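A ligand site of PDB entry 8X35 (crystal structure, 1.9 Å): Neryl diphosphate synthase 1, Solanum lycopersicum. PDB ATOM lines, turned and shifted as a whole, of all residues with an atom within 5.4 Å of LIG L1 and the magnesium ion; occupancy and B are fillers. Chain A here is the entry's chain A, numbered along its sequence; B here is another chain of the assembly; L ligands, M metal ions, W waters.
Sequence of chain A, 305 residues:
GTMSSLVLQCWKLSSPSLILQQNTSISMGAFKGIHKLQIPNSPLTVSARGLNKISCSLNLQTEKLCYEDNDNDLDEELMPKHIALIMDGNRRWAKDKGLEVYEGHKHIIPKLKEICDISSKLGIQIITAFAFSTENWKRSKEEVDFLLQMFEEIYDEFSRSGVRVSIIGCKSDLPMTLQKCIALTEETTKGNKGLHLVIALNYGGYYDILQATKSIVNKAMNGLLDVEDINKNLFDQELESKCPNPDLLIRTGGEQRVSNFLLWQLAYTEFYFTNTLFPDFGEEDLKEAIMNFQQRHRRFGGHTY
Residues that only touch the magnesium ion: Arg 139 (3.9 Å).
Of the 19 residues printed, 2 come within 4 Å of the magnesium ion.
The nearest printed residue that does not touch the magnesium ion is Arg 92 (4.3 Å).
An oxygen (O4) of LIG L1 is in hydrogen-bond range of the backbone NH (N) of Asn 90, 3.3 Å away.
An oxygen (O4) of LIG L1 sits close to the backbone NH (N) of Arg 91, 3.1 Å away.
An oxygen (O2) of LG2 L2 is in hydrogen-bond range of the side-chain amide nitrogen of Asn 136 (3.1 Å).
O2 of LG2 L2 is in salt-bridge range of NH2 of Arg 139, 3.6 Å away.
ND2 of Asn 90 sits close to S1 of LIG L1.
O3 of LIG L1 lies close to NH2 of Arg 299 of chain B, at 3.99 Å.
The guanidinium group (NH1) of Arg 139 lies within salt-bridge range of an oxygen (O6) of LIG L1 (2.7 Å).
O6 of LIG L1 is in hydrogen-bond range of NE2 of His 105.
An oxygen (O6) of LG2 L2 is in salt-bridge range of the guanidinium group (NH2) of Arg 251 (3.4 Å).
The backbone NH (N) of Arg 92 lies within hydrogen-bond range of an oxygen (O1) of LIG L1, 2.9 Å away.
The backbone NH (N) of Gly 89 lies close to a sulfur (S1) of LIG L1 (3.2 Å).
NE of Arg 92 lies within salt-bridge range of O1 of LIG L1 (2.8 Å).
O of Met 87 lies close to S1 of LIG L1, 3.6 Å away.
Residues that only touch LIG L1: Ala 131 (3.1 Å), Asn 136 (3.3 Å), Leu 147 (3.97 Å) and His 303 of chain B (3.8 Å).
Hydrophobic or aromatic side chains within 4 Å of LIG L1: His 105 and Leu 147.
Within 4 Å of LIG L1: Met 87, Asp 88, Gly 89, Asn 90, Arg 91, Arg 92, His 105, Ala 131, Asn 136, Arg 139, Leu 147, Arg 299 of chain B and His 303 of chain B.
The nearest printed residue that does not touch LIG L1 is Glu 143 (4.2 Å).
The side-chain carboxylate (OE2) of Glu 143 lies within salt-bridge range of the guanidinium group (NH1) of Arg 139.
OD2 of Asp 88 lies within salt-bridge range of NH2 of Arg 92.
OE1 of Glu 143 lies within salt-bridge range of NE of Arg 91 (3.6 Å).
ND2 of Asn 90 lies within hydrogen-bond range of O of Met 87 (3.2 Å).
The side-chain carboxylate (OD2) of Asp 88 is in salt-bridge range of the guanidinium group (NH2) of Arg 251, 3.1 Å away.
NE2 of His 303 of chain B is in hydrogen-bond range of NE of Arg 91 (2.9 Å).
The magnesium ion is bound by water W2, O3 of LG2 L2, OD1 of Asp 88, O3 of LIG L1, water W1 and O5 of LIG L1.
The magnesium ion has six donor atoms within binding distance.
Water W2 lies within hydrogen-bond range of O2 of LIG L1 (3.0 Å), NE of Arg 299 of chain B (3.1 Å) and NH2 of Arg 139 (3.4 Å).
Water W1 lies within hydrogen-bond range of an oxygen (O6) of LG2 L2 (2.6 Å), the side-chain carboxylate (OD2) of Asp 88 (2.6 Å) and the guanidinium group (NH2) of Arg 299 of chain B (2.9 Å).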
ATOM      1  N   MET A  87      12.050  -5.176 -31.138  1.00  0.00           N
ATOM      2  CA  MET A  87      12.230  -6.000 -29.923  1.00  0.00           C
ATOM      3  C   MET A  87      10.887  -6.210 -29.223  1.00  0.00           C
ATOM      4  O   MET A  87      10.619  -5.632 -28.174  1.00  0.00           O
ATOM      5  CB  MET A  87      13.212  -5.309 -28.965  1.00  0.00           C
ATOM      6  CG  MET A  87      14.607  -4.960 -29.517  1.00  0.00           C
ATOM      7  SD  MET A  87      15.739  -4.184 -28.289  1.00  0.00           S
ATOM      8  CE  MET A  87      14.921  -2.622 -27.961  1.00  0.00           C
ATOM      9  N   ASP A  88      10.044  -7.060 -29.815  1.00  0.00           N
ATOM     10  CA  ASP A  88       8.630  -7.157 -29.480  1.00  0.00           C
ATOM     11  C   ASP A  88       8.330  -8.445 -28.717  1.00  0.00           C
ATOM     12  O   ASP A  88       9.018  -9.470 -28.848  1.00  0.00           O
ATOM     13  CB  ASP A  88       7.776  -7.098 -30.768  1.00  0.00           C
ATOM     14  CG  ASP A  88       6.289  -6.848 -30.523  1.00  0.00           C
ATOM     15  OD1 ASP A  88       5.927  -6.225 -29.492  1.00  0.00           O
ATOM     16  OD2 ASP A  88       5.463  -7.236 -31.391  1.00  0.00           O
ATOM     17  N   GLY A  89       7.265  -8.402 -27.920  1.00  0.00           N
ATOM     18  CA  GLY A  89       6.774  -9.589 -27.246  1.00  0.00           C
ATOM     19  C   GLY A  89       7.127  -9.726 -25.770  1.00  0.00           C
ATOM     20  O   GLY A  89       7.017 -10.831 -25.222  1.00  0.00           O
ATOM     21  N   ASN A  90       7.501  -8.638 -25.087  1.00  0.00           N
ATOM     22  CA  ASN A  90       8.021  -8.797 -23.738  1.00  0.00           C
ATOM     23  C   ASN A  90       6.911  -8.989 -22.711  1.00  0.00           C
ATOM     24  O   ASN A  90       7.100  -9.723 -21.741  1.00  0.00           O
ATOM     25  CB  ASN A  90       8.875  -7.584 -23.364  1.00  0.00           C
ATOM     26  CG  ASN A  90       9.982  -7.370 -24.338  1.00  0.00           C
ATOM     27  OD1 ASN A  90      10.908  -8.179 -24.411  1.00  0.00           O
ATOM     28  ND2 ASN A  90       9.878  -6.296 -25.123  1.00  0.00           N
ATOM     29  N   ARG A  91       5.764  -8.337 -22.890  1.00  0.00           N
ATOM     30  CA  ARG A  91       4.648  -8.553 -21.974  1.00  0.00           C
ATOM     31  C   ARG A  91       4.112  -9.975 -22.037  1.00  0.00           C
ATOM     32  O   ARG A  91       3.887 -10.613 -20.991  1.00  0.00           O
ATOM     33  CB  ARG A  91       3.521  -7.578 -22.268  1.00  0.00           C
ATOM     34  CG  ARG A  91       3.975  -6.169 -22.398  1.00  0.00           C
ATOM     35  CD  ARG A  91       2.897  -5.257 -22.964  1.00  0.00           C
ATOM     36  NE  ARG A  91       1.925  -4.761 -21.976  1.00  0.00           N
ATOM     37  CZ  ARG A  91       0.989  -5.480 -21.369  1.00  0.00           C
ATOM     38  NH1 ARG A  91       0.754  -6.741 -21.698  1.00  0.00           N
ATOM     39  NH2 ARG A  91       0.241  -4.914 -20.437  1.00  0.00           N
ATOM     40  N   ARG A  92       3.860 -10.468 -23.249  1.00  0.00           N
ATOM     41  CA  ARG A  92       3.350 -11.826 -23.381  1.00  0.00           C
ATOM     42  C   ARG A  92       4.316 -12.829 -22.761  1.00  0.00           C
ATOM     43  O   ARG A  92       3.880 -13.818 -22.148  1.00  0.00           O
ATOM     44  CB  ARG A  92       3.086 -12.149 -24.857  1.00  0.00           C
ATOM     45  CG  ARG A  92       1.779 -11.529 -25.399  1.00  0.00           C
ATOM     46  CD  ARG A  92       1.699 -11.567 -26.952  1.00  0.00           C
ATOM     47  NE  ARG A  92       2.577 -10.566 -27.560  1.00  0.00           N
ATOM     48  CZ  ARG A  92       3.048 -10.639 -28.799  1.00  0.00           C
ATOM     49  NH1 ARG A  92       2.788 -11.667 -29.587  1.00  0.00           N
ATOM     50  NH2 ARG A  92       3.770  -9.623 -29.263  1.00  0.00           N
ATOM     51  N   TRP A  93       5.620 -12.598 -22.902  1.00  0.00           N
ATOM     52  CA  TRP A  93       6.609 -13.479 -22.277  1.00  0.00           C
ATOM     53  C   TRP A  93       6.408 -13.536 -20.763  1.00  0.00           C
ATOM     54  O   TRP A  93       6.430 -14.623 -20.171  1.00  0.00           O
ATOM     55  CB  TRP A  93       8.021 -13.001 -22.610  1.00  0.00           C
ATOM     56  CG  TRP A  93       9.100 -13.845 -22.015  1.00  0.00           C
ATOM     57  CD1 TRP A  93       9.731 -14.903 -22.609  1.00  0.00           C
ATOM     58  CD2 TRP A  93       9.728 -13.667 -20.725  1.00  0.00           C
ATOM     59  NE1 TRP A  93      10.702 -15.405 -21.757  1.00  0.00           N
ATOM     60  CE2 TRP A  93      10.713 -14.665 -20.598  1.00  0.00           C
ATOM     61  CE3 TRP A  93       9.539 -12.776 -19.666  1.00  0.00           C
ATOM     62  CZ2 TRP A  93      11.510 -14.809 -19.447  1.00  0.00           C
ATOM     63  CZ3 TRP A  93      10.337 -12.902 -18.520  1.00  0.00           C
ATOM     64  CH2 TRP A  93      11.310 -13.914 -18.420  1.00  0.00           C
ATOM     65  N   HIS A 105       9.909  -6.434 -19.379  1.00  0.00           N
ATOM     66  CA  HIS A 105      10.615  -5.255 -19.852  1.00  0.00           C
ATOM     67  C   HIS A 105      12.025  -5.179 -19.281  1.00  0.00           C
ATOM     68  O   HIS A 105      12.937  -4.666 -19.946  1.00  0.00           O
ATOM     69  CB  HIS A 105       9.834  -4.007 -19.487  1.00  0.00           C
ATOM     70  CG  HIS A 105       8.584  -3.836 -20.280  1.00  0.00           C
ATOM     71  ND1 HIS A 105       7.421  -3.327 -19.740  1.00  0.00           N
ATOM     72  CD2 HIS A 105       8.313  -4.109 -21.572  1.00  0.00           C
ATOM     73  CE1 HIS A 105       6.497  -3.279 -20.676  1.00  0.00           C
ATOM     74  NE2 HIS A 105       7.008  -3.741 -21.803  1.00  0.00           N
ATOM     75  N   ILE A 108      14.968  -6.242 -21.545  1.00  0.00           N
ATOM     76  CA  ILE A 108      15.231  -5.607 -22.834  1.00  0.00           C
ATOM     77  C   ILE A 108      16.698  -5.185 -22.969  1.00  0.00           C
ATOM     78  O   ILE A 108      17.368  -5.530 -23.957  1.00  0.00           O
ATOM     79  CB  ILE A 108      14.284  -4.412 -23.075  1.00  0.00           C
ATOM     80  CG1 ILE A 108      12.831  -4.878 -23.184  1.00  0.00           C
ATOM     81  CG2 ILE A 108      14.687  -3.660 -24.328  1.00  0.00           C
ATOM     82  CD1 ILE A 108      11.841  -3.744 -23.393  1.00  0.00           C
ATOM     83  N   ALA A 131      13.262   0.639 -29.408  1.00  0.00           N
ATOM     84  CA  ALA A 131      13.006   0.496 -27.980  1.00  0.00           C
ATOM     85  C   ALA A 131      11.719   1.165 -27.514  1.00  0.00           C
ATOM     86  O   ALA A 131      11.135   0.701 -26.528  1.00  0.00           O
ATOM     87  CB  ALA A 131      14.172   1.078 -27.164  1.00  0.00           C
ATOM     88  N   PHE A 132      11.288   2.261 -28.141  1.00  0.00           N
ATOM     89  CA  PHE A 132      10.089   2.993 -27.732  1.00  0.00           C
ATOM     90  C   PHE A 132       9.592   3.799 -28.925  1.00  0.00           C
ATOM     91  O   PHE A 132      10.316   4.670 -29.437  1.00  0.00           O
ATOM     92  CB  PHE A 132      10.395   3.930 -26.534  1.00  0.00           C
ATOM     93  CG  PHE A 132       9.152   4.440 -25.833  1.00  0.00           C
ATOM     94  CD1 PHE A 132       8.573   3.708 -24.802  1.00  0.00           C
ATOM     95  CD2 PHE A 132       8.577   5.655 -26.207  1.00  0.00           C
ATOM     96  CE1 PHE A 132       7.425   4.165 -24.162  1.00  0.00           C
ATOM     97  CE2 PHE A 132       7.436   6.123 -25.561  1.00  0.00           C
ATOM     98  CZ  PHE A 132       6.857   5.378 -24.542  1.00  0.00           C
ATOM     99  N   ASN A 136       3.750   4.444 -28.504  1.00  0.00           N
ATOM    100  CA  ASN A 136       3.732   3.771 -27.194  1.00  0.00           C
ATOM    101  C   ASN A 136       3.337   4.701 -26.044  1.00  0.00           C
ATOM    102  O   ASN A 136       3.123   4.221 -24.924  1.00  0.00           O
ATOM    103  CB  ASN A 136       5.103   3.149 -26.879  1.00  0.00           C
ATOM    104  CG  ASN A 136       5.453   1.953 -27.755  1.00  0.00           C
ATOM    105  OD1 ASN A 136       6.632   1.722 -28.044  1.00  0.00           O
ATOM    106  ND2 ASN A 136       4.435   1.175 -28.181  1.00  0.00           N
ATOM    107  N   ARG A 139       0.066   3.851 -23.928  1.00  0.00           N
ATOM    108  CA  ARG A 139      -0.064   2.882 -22.852  1.00  0.00           C
ATOM    109  C   ARG A 139      -0.327   3.602 -21.521  1.00  0.00           C
ATOM    110  O   ARG A 139      -0.341   4.833 -21.439  1.00  0.00           O
ATOM    111  CB  ARG A 139       1.187   1.997 -22.808  1.00  0.00           C
ATOM    112  CG  ARG A 139       1.478   1.342 -24.158  1.00  0.00           C
ATOM    113  CD  ARG A 139       2.678   0.417 -24.131  1.00  0.00           C
ATOM    114  NE  ARG A 139       2.763  -0.379 -25.364  1.00  0.00           N
ATOM    115  CZ  ARG A 139       3.514  -1.458 -25.529  1.00  0.00           C
ATOM    116  NH1 ARG A 139       4.252  -1.949 -24.532  1.00  0.00           N
ATOM    117  NH2 ARG A 139       3.530  -2.063 -26.716  1.00  0.00           N
ATOM    118  N   GLU A 143       2.898   2.095 -16.878  1.00  0.00           N
ATOM    119  CA  GLU A 143       3.834   1.373 -17.739  1.00  0.00           C
ATOM    120  C   GLU A 143       4.795   2.329 -18.425  1.00  0.00           C
ATOM    121  O   GLU A 143       5.995   2.044 -18.525  1.00  0.00           O
ATOM    122  CB  GLU A 143       3.078   0.532 -18.776  1.00  0.00           C
ATOM    123  CG  GLU A 143       4.012  -0.085 -19.820  1.00  0.00           C
ATOM    124  CD  GLU A 143       3.355  -1.131 -20.717  1.00  0.00           C
ATOM    125  OE1 GLU A 143       2.166  -1.462 -20.515  1.00  0.00           O
ATOM    126  OE2 GLU A 143       4.051  -1.629 -21.640  1.00  0.00           O
ATOM    127  N   LEU A 147       8.975   2.312 -17.921  1.00  0.00           N
ATOM    128  CA  LEU A 147       9.864   2.129 -19.065  1.00  0.00           C
ATOM    129  C   LEU A 147      10.840   3.287 -19.184  1.00  0.00           C
ATOM    130  O   LEU A 147      12.038   3.075 -19.425  1.00  0.00           O
ATOM    131  CB  LEU A 147       9.039   2.000 -20.353  1.00  0.00           C
ATOM    132  CG  LEU A 147       8.465   0.619 -20.719  1.00  0.00           C
ATOM    133  CD1 LEU A 147       7.461   0.725 -21.899  1.00  0.00           C
ATOM    134  CD2 LEU A 147       9.572  -0.360 -21.029  1.00  0.00           C
ATOM    135  N   PHE A 151      14.965   2.937 -18.866  1.00  0.00           N
ATOM    136  CA  PHE A 151      15.953   3.164 -19.925  1.00  0.00           C
ATOM    137  C   PHE A 151      17.204   3.903 -19.442  1.00  0.00           C
ATOM    138  O   PHE A 151      18.168   4.002 -20.200  1.00  0.00           O
ATOM    139  CB  PHE A 151      15.329   3.938 -21.085  1.00  0.00           C
ATOM    140  CG  PHE A 151      14.427   3.087 -21.943  1.00  0.00           C
ATOM    141  CD1 PHE A 151      14.789   1.799 -22.289  1.00  0.00           C
ATOM    142  CD2 PHE A 151      13.208   3.576 -22.383  1.00  0.00           C
ATOM    143  CE1 PHE A 151      13.962   1.008 -23.075  1.00  0.00           C
ATOM    144  CE2 PHE A 151      12.373   2.787 -23.163  1.00  0.00           C
ATOM    145  CZ  PHE A 151      12.757   1.496 -23.514  1.00  0.00           C
ATOM    146  N   ARG A 251      12.078  -9.091 -36.697  1.00  0.00           N
ATOM    147  CA  ARG A 251      11.049  -8.716 -35.723  1.00  0.00           C
ATOM    148  C   ARG A 251      10.616  -9.948 -34.948  1.00  0.00           C
ATOM    149  O   ARG A 251      10.035 -10.879 -35.515  1.00  0.00           O
ATOM    150  CB  ARG A 251       9.828  -8.048 -36.385  1.00  0.00           C
ATOM    151  CG  ARG A 251       8.679  -7.820 -35.381  1.00  0.00           C
ATOM    152  CD  ARG A 251       7.527  -6.940 -35.932  1.00  0.00           C
ATOM    153  NE  ARG A 251       6.552  -6.607 -34.893  1.00  0.00           N
ATOM    154  CZ  ARG A 251       5.877  -5.471 -34.815  1.00  0.00           C
ATOM    155  NH1 ARG A 251       5.997  -4.529 -35.733  1.00  0.00           N
ATOM    156  NH2 ARG A 251       5.057  -5.278 -33.784  1.00  0.00           N
ATOM    157  N   ARG B 299      -2.700  -3.723 -32.711  1.00  0.00           N
ATOM    158  CA  ARG B 299      -2.543  -2.995 -31.450  1.00  0.00           C
ATOM    159  C   ARG B 299      -2.158  -1.529 -31.635  1.00  0.00           C
ATOM    160  O   ARG B 299      -2.383  -0.727 -30.719  1.00  0.00           O
ATOM    161  CB  ARG B 299      -1.511  -3.724 -30.579  1.00  0.00           C
ATOM    162  CG  ARG B 299      -2.074  -5.066 -30.088  1.00  0.00           C
ATOM    163  CD  ARG B 299      -1.457  -5.508 -28.770  1.00  0.00           C
ATOM    164  NE  ARG B 299      -0.258  -6.315 -29.009  1.00  0.00           N
ATOM    165  CZ  ARG B 299      -0.238  -7.459 -29.691  1.00  0.00           C
ATOM    166  NH1 ARG B 299      -1.357  -8.100 -29.996  1.00  0.00           N
ATOM    167  NH2 ARG B 299       0.920  -8.002 -30.051  1.00  0.00           N
ATOM    168  N   HIS B 303      -2.748  -1.064 -26.169  1.00  0.00           N
ATOM    169  CA  HIS B 303      -3.242  -2.367 -25.703  1.00  0.00           C
ATOM    170  C   HIS B 303      -4.760  -2.455 -25.756  1.00  0.00           C
ATOM    171  O   HIS B 303      -5.323  -3.412 -26.294  1.00  0.00           O
ATOM    172  CB  HIS B 303      -2.751  -2.629 -24.275  1.00  0.00           C
ATOM    173  CG  HIS B 303      -1.288  -2.902 -24.204  1.00  0.00           C
ATOM    174  ND1 HIS B 303      -0.395  -2.034 -23.605  1.00  0.00           N
ATOM    175  CD2 HIS B 303      -0.545  -3.926 -24.687  1.00  0.00           C
ATOM    176  CE1 HIS B 303       0.827  -2.527 -23.709  1.00  0.00           C
ATOM    177  NE2 HIS B 303       0.760  -3.669 -24.369  1.00  0.00           N
HETATM  178  O1  LIG L   1       3.800  -8.843 -25.706  1.00  0.00           O
HETATM  179  P1  LIG L   1       3.701  -7.407 -26.135  1.00  0.00           P
HETATM  180  O2  LIG L   1       2.329  -6.863 -25.764  1.00  0.00           O
HETATM  181  O3  LIG L   1       3.999  -7.260 -27.625  1.00  0.00           O
HETATM  182  O4  LIG L   1       4.860  -6.595 -25.305  1.00  0.00           O
HETATM  183  P2  LIG L   1       5.527  -5.160 -25.700  1.00  0.00           P
HETATM  184  O5  LIG L   1       4.745  -4.404 -26.773  1.00  0.00           O
HETATM  185  O6  LIG L   1       5.636  -4.273 -24.485  1.00  0.00           O
HETATM  186  S1  LIG L   1       7.421  -5.501 -26.531  1.00  0.00           S
HETATM  187  C1  LIG L   1       8.051  -4.017 -27.390  1.00  0.00           C
HETATM  188  C2  LIG L   1       8.745  -3.138 -26.344  1.00  0.00           C
HETATM  189  C3  LIG L   1       8.344  -1.901 -26.157  1.00  0.00           C
HETATM  190  C4  LIG L   1       9.030  -1.029 -25.102  1.00  0.00           C
HETATM  191  C5  LIG L   1       7.190  -1.312 -26.969  1.00  0.00           C
HETATM  192  C1  LG2 L   2       6.695  -1.829 -31.938  1.00  0.00           C
HETATM  193  O1  LG2 L   2       6.090  -2.758 -31.069  1.00  0.00           O
HETATM  194  C2  LG2 L   2       7.379  -0.711 -31.127  1.00  0.00           C
HETATM  195  C3  LG2 L   2       8.645  -1.190 -30.424  1.00  0.00           C
HETATM  196  C4  LG2 L   2       9.368  -0.329 -29.691  1.00  0.00           C
HETATM  197  C5  LG2 L   2       9.124  -2.635 -30.544  1.00  0.00           C
HETATM  198  P1  LG2 L   2       4.491  -2.605 -30.702  1.00  0.00           P
HETATM  199  O2  LG2 L   2       4.211  -1.204 -30.178  1.00  0.00           O
HETATM  200  O3  LG2 L   2       4.063  -3.679 -29.714  1.00  0.00           O
HETATM  201  O4  LG2 L   2       3.768  -2.750 -32.168  1.00  0.00           O
HETATM  202  P2  LG2 L   2       2.232  -3.191 -32.435  1.00  0.00           P
HETATM  203  O5  LG2 L   2       2.009  -2.806 -33.897  1.00  0.00           O
HETATM  204  O6  LG2 L   2       2.064  -4.657 -32.210  1.00  0.00           O
HETATM  205  O7  LG2 L   2       1.307  -2.387 -31.569  1.00  0.00           O
HETATM  206 MG    MG M   1       4.088  -5.376 -28.711  1.00  0.00          MG
HETATM  207  O   HOH W   1       3.160  -6.274 -30.520  1.00  0.00           O
HETATM  208  O   HOH W   2       2.327  -4.979 -28.042  1.00  0.00           O
